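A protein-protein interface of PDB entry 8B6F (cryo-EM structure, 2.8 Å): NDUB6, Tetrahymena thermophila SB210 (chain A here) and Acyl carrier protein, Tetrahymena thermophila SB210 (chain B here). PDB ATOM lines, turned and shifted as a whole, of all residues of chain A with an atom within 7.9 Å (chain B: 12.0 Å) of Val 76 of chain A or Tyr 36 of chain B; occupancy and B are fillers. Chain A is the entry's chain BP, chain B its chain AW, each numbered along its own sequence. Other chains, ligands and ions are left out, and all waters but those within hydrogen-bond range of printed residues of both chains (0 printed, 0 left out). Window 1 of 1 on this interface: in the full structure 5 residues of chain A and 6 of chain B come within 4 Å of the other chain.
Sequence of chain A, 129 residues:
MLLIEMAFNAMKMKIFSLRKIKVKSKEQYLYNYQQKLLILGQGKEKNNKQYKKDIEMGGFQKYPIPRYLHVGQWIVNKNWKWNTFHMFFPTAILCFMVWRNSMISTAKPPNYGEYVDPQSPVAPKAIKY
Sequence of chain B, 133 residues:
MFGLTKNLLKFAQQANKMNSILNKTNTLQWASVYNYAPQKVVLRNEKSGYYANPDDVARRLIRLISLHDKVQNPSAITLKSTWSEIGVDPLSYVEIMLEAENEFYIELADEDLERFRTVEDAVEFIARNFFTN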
ATOM      1  N   LYS A  62       3.335   7.363  10.497  1.00  0.00           N
ATOM      2  CA  LYS A  62       1.959   7.449  10.960  1.00  0.00           C
ATOM      3  C   LYS A  62       1.791   6.715  12.285  1.00  0.00           C
ATOM      4  O   LYS A  62       2.351   5.637  12.494  1.00  0.00           O
ATOM      5  CB  LYS A  62       1.014   6.876   9.907  1.00  0.00           C
ATOM      6  CG  LYS A  62       1.151   7.560   8.558  1.00  0.00           C
ATOM      7  CD  LYS A  62       0.103   7.105   7.559  1.00  0.00           C
ATOM      8  CE  LYS A  62       0.281   7.845   6.244  1.00  0.00           C
ATOM      9  NZ  LYS A  62      -0.709   7.439   5.217  1.00  0.00           N
ATOM     10  N   ARG A  67     -10.082   7.367  18.427  1.00  0.00           N
ATOM     11  CA  ARG A  67     -11.321   7.485  17.666  1.00  0.00           C
ATOM     12  C   ARG A  67     -12.214   8.587  18.222  1.00  0.00           C
ATOM     13  O   ARG A  67     -12.842   9.330  17.460  1.00  0.00           O
ATOM     14  CB  ARG A  67     -12.067   6.150  17.670  1.00  0.00           C
ATOM     15  CG  ARG A  67     -11.317   4.993  17.028  1.00  0.00           C
ATOM     16  CD  ARG A  67     -11.412   5.024  15.512  1.00  0.00           C
ATOM     17  NE  ARG A  67     -10.566   6.054  14.921  1.00  0.00           N
ATOM     18  CZ  ARG A  67      -9.294   5.886  14.589  1.00  0.00           C
ATOM     19  NH1 ARG A  67      -8.675   4.732  14.779  1.00  0.00           N
ATOM     20  NH2 ARG A  67      -8.624   6.901  14.054  1.00  0.00           N
ATOM     21  N   GLY A  72      -7.905  16.276  12.836  1.00  0.00           N
ATOM     22  CA  GLY A  72      -7.654  16.174  11.415  1.00  0.00           C
ATOM     23  C   GLY A  72      -6.436  15.372  11.012  1.00  0.00           C
ATOM     24  O   GLY A  72      -6.070  15.394   9.832  1.00  0.00           O
ATOM     25  N   GLN A  73      -5.792  14.663  11.937  1.00  0.00           N
ATOM     26  CA  GLN A  73      -4.591  13.907  11.600  1.00  0.00           C
ATOM     27  C   GLN A  73      -4.895  12.814  10.584  1.00  0.00           C
ATOM     28  O   GLN A  73      -5.581  11.838  10.901  1.00  0.00           O
ATOM     29  CB  GLN A  73      -3.967  13.290  12.855  1.00  0.00           C
ATOM     30  CG  GLN A  73      -3.187  14.265  13.725  1.00  0.00           C
ATOM     31  CD  GLN A  73      -4.068  15.310  14.370  1.00  0.00           C
ATOM     32  OE1 GLN A  73      -5.096  15.700  13.817  1.00  0.00           O
ATOM     33  NE2 GLN A  73      -3.675  15.769  15.551  1.00  0.00           N
ATOM     34  N   TRP A  74      -4.377  12.964   9.367  1.00  0.00           N
ATOM     35  CA  TRP A  74      -4.516  11.956   8.316  1.00  0.00           C
ATOM     36  C   TRP A  74      -5.980  11.597   8.073  1.00  0.00           C
ATOM     37  O   TRP A  74      -6.353  10.424   8.000  1.00  0.00           O
ATOM     38  CB  TRP A  74      -3.704  10.706   8.654  1.00  0.00           C
ATOM     39  CG  TRP A  74      -2.226  10.893   8.550  1.00  0.00           C
ATOM     40  CD1 TRP A  74      -1.508  11.101   7.411  1.00  0.00           C
ATOM     41  CD2 TRP A  74      -1.280  10.875   9.625  1.00  0.00           C
ATOM     42  NE1 TRP A  74      -0.174  11.218   7.709  1.00  0.00           N
ATOM     43  CE2 TRP A  74      -0.007  11.086   9.062  1.00  0.00           C
ATOM     44  CE3 TRP A  74      -1.388  10.706  11.008  1.00  0.00           C
ATOM     45  CZ2 TRP A  74       1.151  11.128   9.832  1.00  0.00           C
ATOM     46  CZ3 TRP A  74      -0.237  10.750  11.773  1.00  0.00           C
ATOM     47  CH2 TRP A  74       1.017  10.961  11.184  1.00  0.00           C
ATOM     48  N   ILE A  75      -6.816  12.619   7.937  1.00  0.00           N
ATOM     49  CA  ILE A  75      -8.236  12.426   7.663  1.00  0.00           C
ATOM     50  C   ILE A  75      -8.444  12.429   6.155  1.00  0.00           C
ATOM     51  O   ILE A  75      -8.057  13.379   5.466  1.00  0.00           O
ATOM     52  CB  ILE A  75      -9.091  13.508   8.341  1.00  0.00           C
ATOM     53  CG1 ILE A  75      -9.124  13.304   9.859  1.00  0.00           C
ATOM     54  CG2 ILE A  75     -10.513  13.520   7.774  1.00  0.00           C
ATOM     55  CD1 ILE A  75      -9.799  12.025  10.321  1.00  0.00           C
ATOM     56  N   VAL A  76      -9.051  11.361   5.643  1.00  0.00           N
ATOM     57  CA  VAL A  76      -9.417  11.244   4.237  1.00  0.00           C
ATOM     58  C   VAL A  76     -10.856  10.755   4.174  1.00  0.00           C
ATOM     59  O   VAL A  76     -11.213   9.779   4.843  1.00  0.00           O
ATOM     60  CB  VAL A  76      -8.475  10.291   3.476  1.00  0.00           C
ATOM     61  CG1 VAL A  76      -8.305   8.991   4.239  1.00  0.00           C
ATOM     62  CG2 VAL A  76      -8.989  10.025   2.068  1.00  0.00           C
ATOM     63  N   ASN A  77     -11.680  11.430   3.378  1.00  0.00           N
ATOM     64  CA  ASN A  77     -13.105  11.146   3.288  1.00  0.00           C
ATOM     65  C   ASN A  77     -13.397  10.425   1.979  1.00  0.00           C
ATOM     66  O   ASN A  77     -12.918  10.838   0.918  1.00  0.00           O
ATOM     67  CB  ASN A  77     -13.921  12.437   3.379  1.00  0.00           C
ATOM     68  CG  ASN A  77     -15.398  12.181   3.590  1.00  0.00           C
ATOM     69  OD1 ASN A  77     -15.940  11.176   3.136  1.00  0.00           O
ATOM     70  ND2 ASN A  77     -16.061  13.097   4.286  1.00  0.00           N
ATOM     71  N   LYS A  78     -14.179   9.347   2.062  1.00  0.00           N
ATOM     72  CA  LYS A  78     -14.526   8.578   0.870  1.00  0.00           C
ATOM     73  C   LYS A  78     -15.409   9.380  -0.075  1.00  0.00           C
ATOM     74  O   LYS A  78     -15.265   9.286  -1.300  1.00  0.00           O
ATOM     75  CB  LYS A  78     -15.226   7.281   1.271  1.00  0.00           C
ATOM     76  CG  LYS A  78     -14.306   6.232   1.870  1.00  0.00           C
ATOM     77  CD  LYS A  78     -13.407   5.630   0.806  1.00  0.00           C
ATOM     78  CE  LYS A  78     -12.802   4.319   1.276  1.00  0.00           C
ATOM     79  NZ  LYS A  78     -11.975   3.681   0.213  1.00  0.00           N
ATOM     80  N   ASN A  79     -16.339  10.165   0.471  1.00  0.00           N
ATOM     81  CA  ASN A  79     -17.303  10.917  -0.322  1.00  0.00           C
ATOM     82  C   ASN A  79     -16.820  12.324  -0.638  1.00  0.00           C
ATOM     83  O   ASN A  79     -17.640  13.235  -0.813  1.00  0.00           O
ATOM     84  CB  ASN A  79     -18.645  10.968   0.411  1.00  0.00           C
ATOM     85  CG  ASN A  79     -19.804  11.291  -0.511  1.00  0.00           C
ATOM     86  OD1 ASN A  79     -19.770  10.984  -1.701  1.00  0.00           O
ATOM     87  ND2 ASN A  79     -20.842  11.911   0.040  1.00  0.00           N
ATOM     88  N   TRP A  80     -15.503  12.529  -0.717  1.00  0.00           N
ATOM     89  CA  TRP A  80     -14.976  13.876  -0.898  1.00  0.00           C
ATOM     90  C   TRP A  80     -15.417  14.485  -2.222  1.00  0.00           C
ATOM     91  O   TRP A  80     -15.537  15.710  -2.328  1.00  0.00           O
ATOM     92  CB  TRP A  80     -13.448  13.866  -0.796  1.00  0.00           C
ATOM     93  CG  TRP A  80     -12.741  13.152  -1.908  1.00  0.00           C
ATOM     94  CD1 TRP A  80     -12.350  11.845  -1.925  1.00  0.00           C
ATOM     95  CD2 TRP A  80     -12.324  13.710  -3.161  1.00  0.00           C
ATOM     96  NE1 TRP A  80     -11.722  11.554  -3.112  1.00  0.00           N
ATOM     97  CE2 TRP A  80     -11.693  12.683  -3.887  1.00  0.00           C
ATOM     98  CE3 TRP A  80     -12.426  14.980  -3.736  1.00  0.00           C
ATOM     99  CZ2 TRP A  80     -11.169  12.884  -5.161  1.00  0.00           C
ATOM    100  CZ3 TRP A  80     -11.905  15.179  -5.002  1.00  0.00           C
ATOM    101  CH2 TRP A  80     -11.284  14.136  -5.701  1.00  0.00           C
ATOM    102  N   TYR B  36      -7.416   2.036   5.307  1.00  0.00           N
ATOM    103  CA  TYR B  36      -8.004   2.977   6.300  1.00  0.00           C
ATOM    104  C   TYR B  36      -8.086   2.326   7.671  1.00  0.00           C
ATOM    105  O   TYR B  36      -8.294   1.119   7.783  1.00  0.00           O
ATOM    106  CB  TYR B  36      -9.395   3.432   5.857  1.00  0.00           C
ATOM    107  CG  TYR B  36      -9.425   4.074   4.492  1.00  0.00           C
ATOM    108  CD1 TYR B  36      -9.527   3.302   3.343  1.00  0.00           C
ATOM    109  CD2 TYR B  36      -9.359   5.453   4.351  1.00  0.00           C
ATOM    110  CE1 TYR B  36      -9.557   3.883   2.093  1.00  0.00           C
ATOM    111  CE2 TYR B  36      -9.389   6.044   3.104  1.00  0.00           C
ATOM    112  CZ  TYR B  36      -9.488   5.255   1.980  1.00  0.00           C
ATOM    113  OH  TYR B  36      -9.519   5.838   0.735  1.00  0.00           O
ATOM    114  N   ALA B  37      -7.918   3.131   8.713  1.00  0.00           N
ATOM    115  CA  ALA B  37      -8.013   2.614  10.067  1.00  0.00           C
ATOM    116  C   ALA B  37      -9.448   2.176  10.355  1.00  0.00           C
ATOM    117  O   ALA B  37     -10.397   2.871   9.979  1.00  0.00           O
ATOM    118  CB  ALA B  37      -7.577   3.673  11.077  1.00  0.00           C
ATOM    119  N   PRO B  38      -9.645   1.034  11.012  1.00  0.00           N
ATOM    120  CA  PRO B  38     -11.010   0.597  11.318  1.00  0.00           C
ATOM    121  C   PRO B  38     -11.667   1.502  12.344  1.00  0.00           C
ATOM    122  O   PRO B  38     -11.004   2.128  13.172  1.00  0.00           O
ATOM    123  CB  PRO B  38     -10.814  -0.820  11.870  1.00  0.00           C
ATOM    124  CG  PRO B  38      -9.444  -0.805  12.442  1.00  0.00           C
ATOM    125  CD  PRO B  38      -8.637   0.111  11.563  1.00  0.00           C
ATOM    126  N   GLN B  39     -12.999   1.562  12.281  1.00  0.00           N
ATOM    127  CA  GLN B  39     -13.746   2.370  13.236  1.00  0.00           C
ATOM    128  C   GLN B  39     -13.612   1.844  14.659  1.00  0.00           C
ATOM    129  O   GLN B  39     -13.908   2.575  15.609  1.00  0.00           O
ATOM    130  CB  GLN B  39     -15.222   2.419  12.840  1.00  0.00           C
ATOM    131  CG  GLN B  39     -15.479   3.012  11.460  1.00  0.00           C
ATOM    132  CD  GLN B  39     -15.108   4.480  11.368  1.00  0.00           C
ATOM    133  OE1 GLN B  39     -14.717   5.099  12.355  1.00  0.00           O
ATOM    134  NE2 GLN B  39     -15.234   5.047  10.173  1.00  0.00           N
ATOM    135  N   LYS B  40     -13.181   0.598  14.829  1.00  0.00           N
ATOM    136  CA  LYS B  40     -12.985   0.044  16.157  1.00  0.00           C
ATOM    137  C   LYS B  40     -11.718   0.613  16.792  1.00  0.00           C
ATOM    138  O   LYS B  40     -10.820   1.118  16.112  1.00  0.00           O
ATOM    139  CB  LYS B  40     -12.902  -1.481  16.095  1.00  0.00           C
ATOM    140  CG  LYS B  40     -14.254  -2.177  16.001  1.00  0.00           C
ATOM    141  CD  LYS B  40     -15.033  -1.756  14.761  1.00  0.00           C
ATOM    142  CE  LYS B  40     -16.320  -2.555  14.623  1.00  0.00           C
ATOM    143  NZ  LYS B  40     -17.114  -2.131  13.435  1.00  0.00           N
ATOM    144  N   VAL B  41     -11.653   0.525  18.120  1.00  0.00           N
ATOM    145  CA  VAL B  41     -10.517   1.066  18.854  1.00  0.00           C
ATOM    146  C   VAL B  41      -9.299   0.181  18.633  1.00  0.00           C
ATOM    147  O   VAL B  41      -9.349  -1.039  18.840  1.00  0.00           O
ATOM    148  CB  VAL B  41     -10.853   1.189  20.348  1.00  0.00           C
ATOM    149  CG1 VAL B  41      -9.623   1.599  21.148  1.00  0.00           C
ATOM    150  CG2 VAL B  41     -11.980   2.185  20.556  1.00  0.00           C
ATOM    151  N   VAL B  42      -8.194   0.795  18.216  1.00  0.00           N
ATOM    152  CA  VAL B  42      -6.934   0.102  17.980  1.00  0.00           C
ATOM    153  C   VAL B  42      -5.869   0.731  18.866  1.00  0.00           C
ATOM    154  O   VAL B  42      -5.788   1.959  18.976  1.00  0.00           O
ATOM    155  CB  VAL B  42      -6.516   0.165  16.496  1.00  0.00           C
ATOM    156  CG1 VAL B  42      -5.232  -0.617  16.266  1.00  0.00           C
ATOM    157  CG2 VAL B  42      -7.632  -0.358  15.605  1.00  0.00           C
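Of the 11 printed residues of chain A, 3 touch a printed residue of chain B.
Printed residues of chain A that touch a printed residue of chain B: Arg 67, Val 76 and Lys 78.
Hydrophobic or aromatic side chains of chain A within 4 Å of the printed part of chain B: Val 76.
Of the 7 printed residues of chain B, 4 touch a printed residue of chain A.
Printed residues of chain B that touch a printed residue of chain A: Tyr 36, Pro 38, Gln 39 and Lys 40.
Among the printed residues, 5 pairs touch across the chains.
Among the printed residues, no Asp or Glu carboxylate lies within 4 Å of a Lys or Arg side-chain nitrogen of the other chain.
Arg 67 of chain A touches Pro 38 of chain B (CD to O, 3.7 Å).
Gln 39 of chain B touches Arg 67 of chain A (O to CD, 3.5 Å).
Arg 67 of chain A touches Lys 40 of chain B (CD to O, 3.996 Å).
CE2 of Tyr 36 of chain B touches CG1 of Val 76 of chain A, at 3.3 Å.
The side-chain hydroxyl (OH) of Tyr 36 of chain B lies close to the side-chain amino group (NZ) of Lys 78 of chain A (3.3 Å).
Val 76 of chain A touches just one residue of chain B: Tyr 36 (3.3 Å).
Tyr 36 of chain B touches just these residues of chain A: Val 76 (3.3 Å) and Lys 78 (3.1 Å).
No residue of chain B comes within 4 Å of Ile 75 of chain A.
No residue of chain B comes within 4 Å of Asn 77 of chain A.
Of chain B, only Tyr 36 comes within 4 Å of Lys 78 of chain A.
Printed residues of chain A within 4 Å of Gln 39 of chain B: Arg 67 (3.5 Å).
Of the printed residues of chain B, Arg 67 of chain A touches Pro 38 (3.7 Å), Gln 39 (3.5 Å) and Lys 40 (3.996 Å).
Of the printed residues of chain A, Lys 40 of chain B touches Arg 67.
Asn 79 of chain A touches none of the printed residues of chain B.
The nearest printed residue of chain A that does not touch Gln 39 of chain B is Val 76 of chain A (8.2 Å).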
